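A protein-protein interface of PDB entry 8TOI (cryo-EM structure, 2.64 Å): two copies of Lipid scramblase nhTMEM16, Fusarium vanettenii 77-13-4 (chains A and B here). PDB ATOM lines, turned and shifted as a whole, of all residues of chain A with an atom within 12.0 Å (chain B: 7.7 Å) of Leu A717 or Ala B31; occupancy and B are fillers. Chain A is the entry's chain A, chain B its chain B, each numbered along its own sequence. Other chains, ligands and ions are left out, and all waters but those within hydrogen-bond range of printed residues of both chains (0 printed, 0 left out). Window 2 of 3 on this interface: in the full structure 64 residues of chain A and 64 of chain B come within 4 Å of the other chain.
Of the printed residues of chain B, Leu A717 touches Ala B31 (3.998 Å), Arg B34 (3.7 Å) and Glu B63 (3.5 Å).
Printed residues of chain A within 4 Å of Ala B31: Leu A717 (3.998 Å).
No residue of chain A comes within 4 Å of Pro B30.
No residue of chain A comes within 4 Å of Ala B32.
No residue of chain A comes within 4 Å of Glu B33.
Arg B34 touches just these residues of chain A: Ile A713 and Leu A717.
Of chain A, only Gln A716 (3.3 Å) and Leu A717 (3.5 Å) come within 4 Å of Glu B63.
Printed residues of chain A within 4 Å of His B59: Met A712 (3.4 Å), Gln A715 (3.1 Å) and Gln A716 (3.5 Å).
Printed residues of chain B within 4 Å of Ile A713: Arg B34 (3.8 Å).
Of the printed residues of chain B, Gln A715 touches His B59.
Printed residues of chain B within 4 Å of Gln A716: His B59 and Glu B63.
Of the printed residues of chain B, Met A712 touches His B59 (3.4 Å).
Ala A719 touches none of the printed residues of chain B.
The nearest printed residue of chain A that does not touch Ala B31 is Ile A713 (8.0 Å).
The nearest printed residue of chain A that does not touch His B59 is Ile A713 (5.5 Å).
No position is printed for both chains.
The side-chain carboxylate (OD1) of Asp B35 is in salt-bridge range of the guanidinium group (NH2) of Arg B34.
Of the 11 printed residues of chain B, 4 touch a printed residue of chain A.
Among the printed residues, 8 pairs touch across the chains.
The side-chain amide nitrogen (NE2) of Gln A715 lies within hydrogen-bond range of a ring nitrogen (NE2) of His B59.
NE2 of Gln A716 is in hydrogen-bond range of ND1 of His B59 (3.5 Å).
The side-chain amide oxygen (OE1) of Gln A716 sits close to the side-chain carboxylate (OE1) of Glu B63, 3.4 Å away.
Among the printed residues, merely in contact across the chains: Met A712 with His B59 (3.4 Å), Leu A717 with Glu B63 (3.5 Å), Leu A717 with Arg B34 (3.7 Å), Ile A713 with Arg B34 (3.8 Å) and Leu A717 with Ala B31 (3.998 Å).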
ATOM      1  N   ILE A 708     -15.757 -17.067 -10.556  1.00  0.00           N
ATOM      2  CA  ILE A 708     -17.064 -17.299 -11.175  1.00  0.00           C
ATOM      3  C   ILE A 708     -17.575 -18.711 -10.871  1.00  0.00           C
ATOM      4  O   ILE A 708     -18.788 -18.916 -10.730  1.00  0.00           O
ATOM      5  CB  ILE A 708     -17.026 -16.967 -12.679  1.00  0.00           C
ATOM      6  CG1 ILE A 708     -16.624 -15.502 -12.858  1.00  0.00           C
ATOM      7  CG2 ILE A 708     -18.389 -17.150 -13.335  1.00  0.00           C
ATOM      8  CD1 ILE A 708     -17.590 -14.513 -12.219  1.00  0.00           C
ATOM      9  N   GLY A 709     -16.680 -19.688 -10.693  1.00  0.00           N
ATOM     10  CA  GLY A 709     -17.117 -20.991 -10.212  1.00  0.00           C
ATOM     11  C   GLY A 709     -17.661 -20.944  -8.797  1.00  0.00           C
ATOM     12  O   GLY A 709     -18.678 -21.578  -8.490  1.00  0.00           O
ATOM     13  N   ARG A 710     -17.015 -20.160  -7.927  1.00  0.00           N
ATOM     14  CA  ARG A 710     -17.518 -19.970  -6.570  1.00  0.00           C
ATOM     15  C   ARG A 710     -18.845 -19.218  -6.568  1.00  0.00           C
ATOM     16  O   ARG A 710     -19.729 -19.513  -5.759  1.00  0.00           O
ATOM     17  CB  ARG A 710     -16.473 -19.228  -5.740  1.00  0.00           C
ATOM     18  CG  ARG A 710     -15.339 -20.118  -5.271  1.00  0.00           C
ATOM     19  CD  ARG A 710     -14.270 -19.328  -4.547  1.00  0.00           C
ATOM     20  NE  ARG A 710     -13.282 -20.207  -3.934  1.00  0.00           N
ATOM     21  CZ  ARG A 710     -12.023 -19.868  -3.699  1.00  0.00           C
ATOM     22  NH1 ARG A 710     -11.557 -18.674  -4.027  1.00  0.00           N
ATOM     23  NH2 ARG A 710     -11.210 -20.749  -3.126  1.00  0.00           N
ATOM     24  N   ARG A 711     -19.007 -18.257  -7.482  1.00  0.00           N
ATOM     25  CA  ARG A 711     -20.264 -17.522  -7.588  1.00  0.00           C
ATOM     26  C   ARG A 711     -21.384 -18.408  -8.116  1.00  0.00           C
ATOM     27  O   ARG A 711     -22.534 -18.286  -7.683  1.00  0.00           O
ATOM     28  CB  ARG A 711     -20.080 -16.301  -8.487  1.00  0.00           C
ATOM     29  N   MET A 712     -21.066 -19.304  -9.055  1.00  0.00           N
ATOM     30  CA  MET A 712     -22.058 -20.253  -9.552  1.00  0.00           C
ATOM     31  C   MET A 712     -22.456 -21.250  -8.473  1.00  0.00           C
ATOM     32  O   MET A 712     -23.621 -21.655  -8.397  1.00  0.00           O
ATOM     33  CB  MET A 712     -21.522 -20.988 -10.781  1.00  0.00           C
ATOM     34  CG  MET A 712     -21.564 -20.192 -12.073  1.00  0.00           C
ATOM     35  SD  MET A 712     -20.715 -21.048 -13.413  1.00  0.00           S
ATOM     36  CE  MET A 712     -21.050 -19.952 -14.789  1.00  0.00           C
ATOM     37  N   ILE A 713     -21.500 -21.657  -7.634  1.00  0.00           N
ATOM     38  CA  ILE A 713     -21.813 -22.518  -6.497  1.00  0.00           C
ATOM     39  C   ILE A 713     -22.699 -21.781  -5.493  1.00  0.00           C
ATOM     40  O   ILE A 713     -23.690 -22.330  -4.995  1.00  0.00           O
ATOM     41  CB  ILE A 713     -20.511 -23.034  -5.854  1.00  0.00           C
ATOM     42  CG1 ILE A 713     -19.900 -24.137  -6.718  1.00  0.00           C
ATOM     43  CG2 ILE A 713     -20.742 -23.554  -4.444  1.00  0.00           C
ATOM     44  CD1 ILE A 713     -18.563 -24.628  -6.221  1.00  0.00           C
ATOM     45  N   GLU A 714     -22.378 -20.512  -5.216  1.00  0.00           N
ATOM     46  CA  GLU A 714     -23.116 -19.741  -4.219  1.00  0.00           C
ATOM     47  C   GLU A 714     -24.533 -19.413  -4.685  1.00  0.00           C
ATOM     48  O   GLU A 714     -25.478 -19.471  -3.889  1.00  0.00           O
ATOM     49  CB  GLU A 714     -22.357 -18.460  -3.882  1.00  0.00           C
ATOM     50  N   GLN A 715     -24.705 -19.066  -5.960  1.00  0.00           N
ATOM     51  CA  GLN A 715     -26.034 -18.791  -6.488  1.00  0.00           C
ATOM     52  C   GLN A 715     -26.766 -20.051  -6.920  1.00  0.00           C
ATOM     53  O   GLN A 715     -27.961 -19.983  -7.228  1.00  0.00           O
ATOM     54  CB  GLN A 715     -25.952 -17.812  -7.665  1.00  0.00           C
ATOM     55  CG  GLN A 715     -25.601 -18.442  -9.002  1.00  0.00           C
ATOM     56  CD  GLN A 715     -25.602 -17.430 -10.130  1.00  0.00           C
ATOM     57  OE1 GLN A 715     -26.088 -16.312  -9.975  1.00  0.00           O
ATOM     58  NE2 GLN A 715     -25.054 -17.819 -11.274  1.00  0.00           N
ATOM     59  N   GLN A 716     -26.081 -21.195  -6.950  1.00  0.00           N
ATOM     60  CA  GLN A 716     -26.746 -22.461  -7.223  1.00  0.00           C
ATOM     61  C   GLN A 716     -27.622 -22.888  -6.053  1.00  0.00           C
ATOM     62  O   GLN A 716     -28.679 -23.497  -6.254  1.00  0.00           O
ATOM     63  CB  GLN A 716     -25.703 -23.531  -7.540  1.00  0.00           C
ATOM     64  CG  GLN A 716     -26.254 -24.776  -8.197  1.00  0.00           C
ATOM     65  CD  GLN A 716     -25.193 -25.533  -8.964  1.00  0.00           C
ATOM     66  OE1 GLN A 716     -24.996 -26.729  -8.759  1.00  0.00           O
ATOM     67  NE2 GLN A 716     -24.503 -24.839  -9.858  1.00  0.00           N
ATOM     68  N   LEU A 717     -27.200 -22.579  -4.828  1.00  0.00           N
ATOM     69  CA  LEU A 717     -27.967 -22.892  -3.630  1.00  0.00           C
ATOM     70  C   LEU A 717     -28.722 -21.684  -3.088  1.00  0.00           C
ATOM     71  O   LEU A 717     -29.305 -21.761  -2.002  1.00  0.00           O
ATOM     72  CB  LEU A 717     -27.048 -23.469  -2.555  1.00  0.00           C
ATOM     73  CG  LEU A 717     -26.437 -24.826  -2.903  1.00  0.00           C
ATOM     74  CD1 LEU A 717     -25.440 -25.249  -1.843  1.00  0.00           C
ATOM     75  CD2 LEU A 717     -27.522 -25.875  -3.073  1.00  0.00           C
ATOM     76  N   ALA A 718     -28.722 -20.571  -3.819  1.00  0.00           N
ATOM     77  CA  ALA A 718     -29.467 -19.386  -3.418  1.00  0.00           C
ATOM     78  C   ALA A 718     -30.943 -19.461  -3.781  1.00  0.00           C
ATOM     79  O   ALA A 718     -31.713 -18.592  -3.358  1.00  0.00           O
ATOM     80  CB  ALA A 718     -28.852 -18.132  -4.047  1.00  0.00           C
ATOM     81  N   ALA A 719     -31.352 -20.465  -4.549  1.00  0.00           N
ATOM     82  CA  ALA A 719     -32.751 -20.629  -4.920  1.00  0.00           C
ATOM     83  C   ALA A 719     -33.177 -22.085  -4.778  1.00  0.00           C
ATOM     84  O   ALA A 719     -32.340 -22.974  -4.624  1.00  0.00           O
ATOM     85  CB  ALA A 719     -32.985 -20.141  -6.340  1.00  0.00           C
ATOM     86  N   LYS B  28     -20.026 -32.899  -9.957  1.00  0.00           N
ATOM     87  CA  LYS B  28     -21.160 -32.576  -9.102  1.00  0.00           C
ATOM     88  C   LYS B  28     -20.682 -32.021  -7.762  1.00  0.00           C
ATOM     89  O   LYS B  28     -19.656 -32.439  -7.222  1.00  0.00           O
ATOM     90  CB  LYS B  28     -22.056 -33.802  -8.893  1.00  0.00           C
ATOM     91  CG  LYS B  28     -21.425 -34.963  -8.145  1.00  0.00           C
ATOM     92  CD  LYS B  28     -22.411 -36.105  -7.973  1.00  0.00           C
ATOM     93  CE  LYS B  28     -22.652 -36.839  -9.277  1.00  0.00           C
ATOM     94  NZ  LYS B  28     -23.513 -38.038  -9.086  1.00  0.00           N
ATOM     95  N   VAL B  29     -21.405 -31.026  -7.256  1.00  0.00           N
ATOM     96  CA  VAL B  29     -21.075 -30.389  -5.984  1.00  0.00           C
ATOM     97  C   VAL B  29     -22.276 -30.556  -5.060  1.00  0.00           C
ATOM     98  O   VAL B  29     -23.218 -29.753  -5.119  1.00  0.00           O
ATOM     99  CB  VAL B  29     -20.708 -28.907  -6.166  1.00  0.00           C
ATOM    100  CG1 VAL B  29     -20.329 -28.273  -4.831  1.00  0.00           C
ATOM    101  CG2 VAL B  29     -19.575 -28.743  -7.165  1.00  0.00           C
ATOM    102  N   PRO B  30     -22.309 -31.594  -4.228  1.00  0.00           N
ATOM    103  CA  PRO B  30     -23.431 -31.752  -3.297  1.00  0.00           C
ATOM    104  C   PRO B  30     -23.372 -30.733  -2.172  1.00  0.00           C
ATOM    105  O   PRO B  30     -22.308 -30.217  -1.821  1.00  0.00           O
ATOM    106  CB  PRO B  30     -23.260 -33.179  -2.768  1.00  0.00           C
ATOM    107  CG  PRO B  30     -21.826 -33.492  -2.966  1.00  0.00           C
ATOM    108  CD  PRO B  30     -21.361 -32.719  -4.159  1.00  0.00           C
ATOM    109  N   ALA B  31     -24.546 -30.442  -1.608  1.00  0.00           N
ATOM    110  CA  ALA B  31     -24.651 -29.380  -0.613  1.00  0.00           C
ATOM    111  C   ALA B  31     -24.089 -29.797   0.740  1.00  0.00           C
ATOM    112  O   ALA B  31     -23.624 -28.941   1.503  1.00  0.00           O
ATOM    113  CB  ALA B  31     -26.108 -28.943  -0.467  1.00  0.00           C
ATOM    114  N   ALA B  32     -24.125 -31.091   1.062  1.00  0.00           N
ATOM    115  CA  ALA B  32     -23.705 -31.542   2.383  1.00  0.00           C
ATOM    116  C   ALA B  32     -22.192 -31.531   2.569  1.00  0.00           C
ATOM    117  O   ALA B  32     -21.728 -31.394   3.705  1.00  0.00           O
ATOM    118  CB  ALA B  32     -24.257 -32.941   2.664  1.00  0.00           C
ATOM    119  N   GLU B  33     -21.416 -31.668   1.497  1.00  0.00           N
ATOM    120  CA  GLU B  33     -19.958 -31.574   1.565  1.00  0.00           C
ATOM    121  C   GLU B  33     -19.459 -30.521   0.579  1.00  0.00           C
ATOM    122  O   GLU B  33     -18.529 -30.743  -0.199  1.00  0.00           O
ATOM    123  CB  GLU B  33     -19.289 -32.934   1.329  1.00  0.00           C
ATOM    124  CG  GLU B  33     -19.713 -33.712   0.079  1.00  0.00           C
ATOM    125  CD  GLU B  33     -20.887 -34.634   0.314  1.00  0.00           C
ATOM    126  OE1 GLU B  33     -21.983 -34.133   0.624  1.00  0.00           O
ATOM    127  OE2 GLU B  33     -20.711 -35.863   0.188  1.00  0.00           O
ATOM    128  N   ARG B  34     -20.092 -29.342   0.629  1.00  0.00           N
ATOM    129  CA  ARG B  34     -19.839 -28.279  -0.343  1.00  0.00           C
ATOM    130  C   ARG B  34     -18.416 -27.737  -0.277  1.00  0.00           C
ATOM    131  O   ARG B  34     -17.727 -27.709  -1.305  1.00  0.00           O
ATOM    132  CB  ARG B  34     -20.822 -27.133  -0.125  1.00  0.00           C
ATOM    133  CG  ARG B  34     -20.564 -25.934  -1.014  1.00  0.00           C
ATOM    134  CD  ARG B  34     -21.787 -25.041  -1.108  1.00  0.00           C
ATOM    135  NE  ARG B  34     -21.919 -24.163   0.048  1.00  0.00           N
ATOM    136  CZ  ARG B  34     -21.251 -23.029   0.215  1.00  0.00           C
ATOM    137  NH1 ARG B  34     -20.401 -22.585  -0.697  1.00  0.00           N
ATOM    138  NH2 ARG B  34     -21.447 -22.316   1.320  1.00  0.00           N
ATOM    139  N   ASP B  35     -17.963 -27.328   0.914  1.00  0.00           N
ATOM    140  CA  ASP B  35     -16.676 -26.651   1.074  1.00  0.00           C
ATOM    141  C   ASP B  35     -15.512 -27.556   0.694  1.00  0.00           C
ATOM    142  O   ASP B  35     -14.617 -27.144  -0.055  1.00  0.00           O
ATOM    143  CB  ASP B  35     -16.522 -26.161   2.514  1.00  0.00           C
ATOM    144  CG  ASP B  35     -17.655 -25.254   2.943  1.00  0.00           C
ATOM    145  OD1 ASP B  35     -18.247 -24.588   2.070  1.00  0.00           O
ATOM    146  OD2 ASP B  35     -17.956 -25.210   4.155  1.00  0.00           O
ATOM    147  N   ALA B  37     -15.806 -29.943  -1.333  1.00  0.00           N
ATOM    148  CA  ALA B  37     -15.879 -29.958  -2.788  1.00  0.00           C
ATOM    149  C   ALA B  37     -15.258 -28.701  -3.379  1.00  0.00           C
ATOM    150  O   ALA B  37     -14.417 -28.789  -4.285  1.00  0.00           O
ATOM    151  CB  ALA B  37     -17.330 -30.096  -3.244  1.00  0.00           C
ATOM    152  N   HIS B  59     -22.612 -23.752 -15.750  1.00  0.00           N
ATOM    153  CA  HIS B  59     -23.600 -24.336 -14.857  1.00  0.00           C
ATOM    154  C   HIS B  59     -23.915 -25.771 -15.253  1.00  0.00           C
ATOM    155  O   HIS B  59     -23.939 -26.128 -16.434  1.00  0.00           O
ATOM    156  CB  HIS B  59     -24.882 -23.510 -14.868  1.00  0.00           C
ATOM    157  CG  HIS B  59     -24.892 -22.397 -13.871  1.00  0.00           C
ATOM    158  ND1 HIS B  59     -24.951 -22.616 -12.512  1.00  0.00           N
ATOM    159  CD2 HIS B  59     -24.852 -21.054 -14.035  1.00  0.00           C
ATOM    160  CE1 HIS B  59     -24.946 -21.455 -11.882  1.00  0.00           C
ATOM    161  NE2 HIS B  59     -24.887 -20.492 -12.783  1.00  0.00           N
ATOM    162  N   GLU B  63     -27.761 -29.969  -9.655  1.00  0.00           N
ATOM    163  CA  GLU B  63     -26.777 -29.557  -8.644  1.00  0.00           C
ATOM    164  C   GLU B  63     -25.382 -30.087  -9.008  1.00  0.00           C
ATOM    165  O   GLU B  63     -24.827 -31.004  -8.399  1.00  0.00           O
ATOM    166  CB  GLU B  63     -27.251 -29.974  -7.238  1.00  0.00           C
ATOM    167  CG  GLU B  63     -26.374 -29.570  -6.044  1.00  0.00           C
ATOM    168  CD  GLU B  63     -26.297 -28.067  -5.836  1.00  0.00           C
ATOM    169  OE1 GLU B  63     -27.237 -27.350  -6.239  1.00  0.00           O
ATOM    170  OE2 GLU B  63     -25.289 -27.600  -5.264  1.00  0.00           O
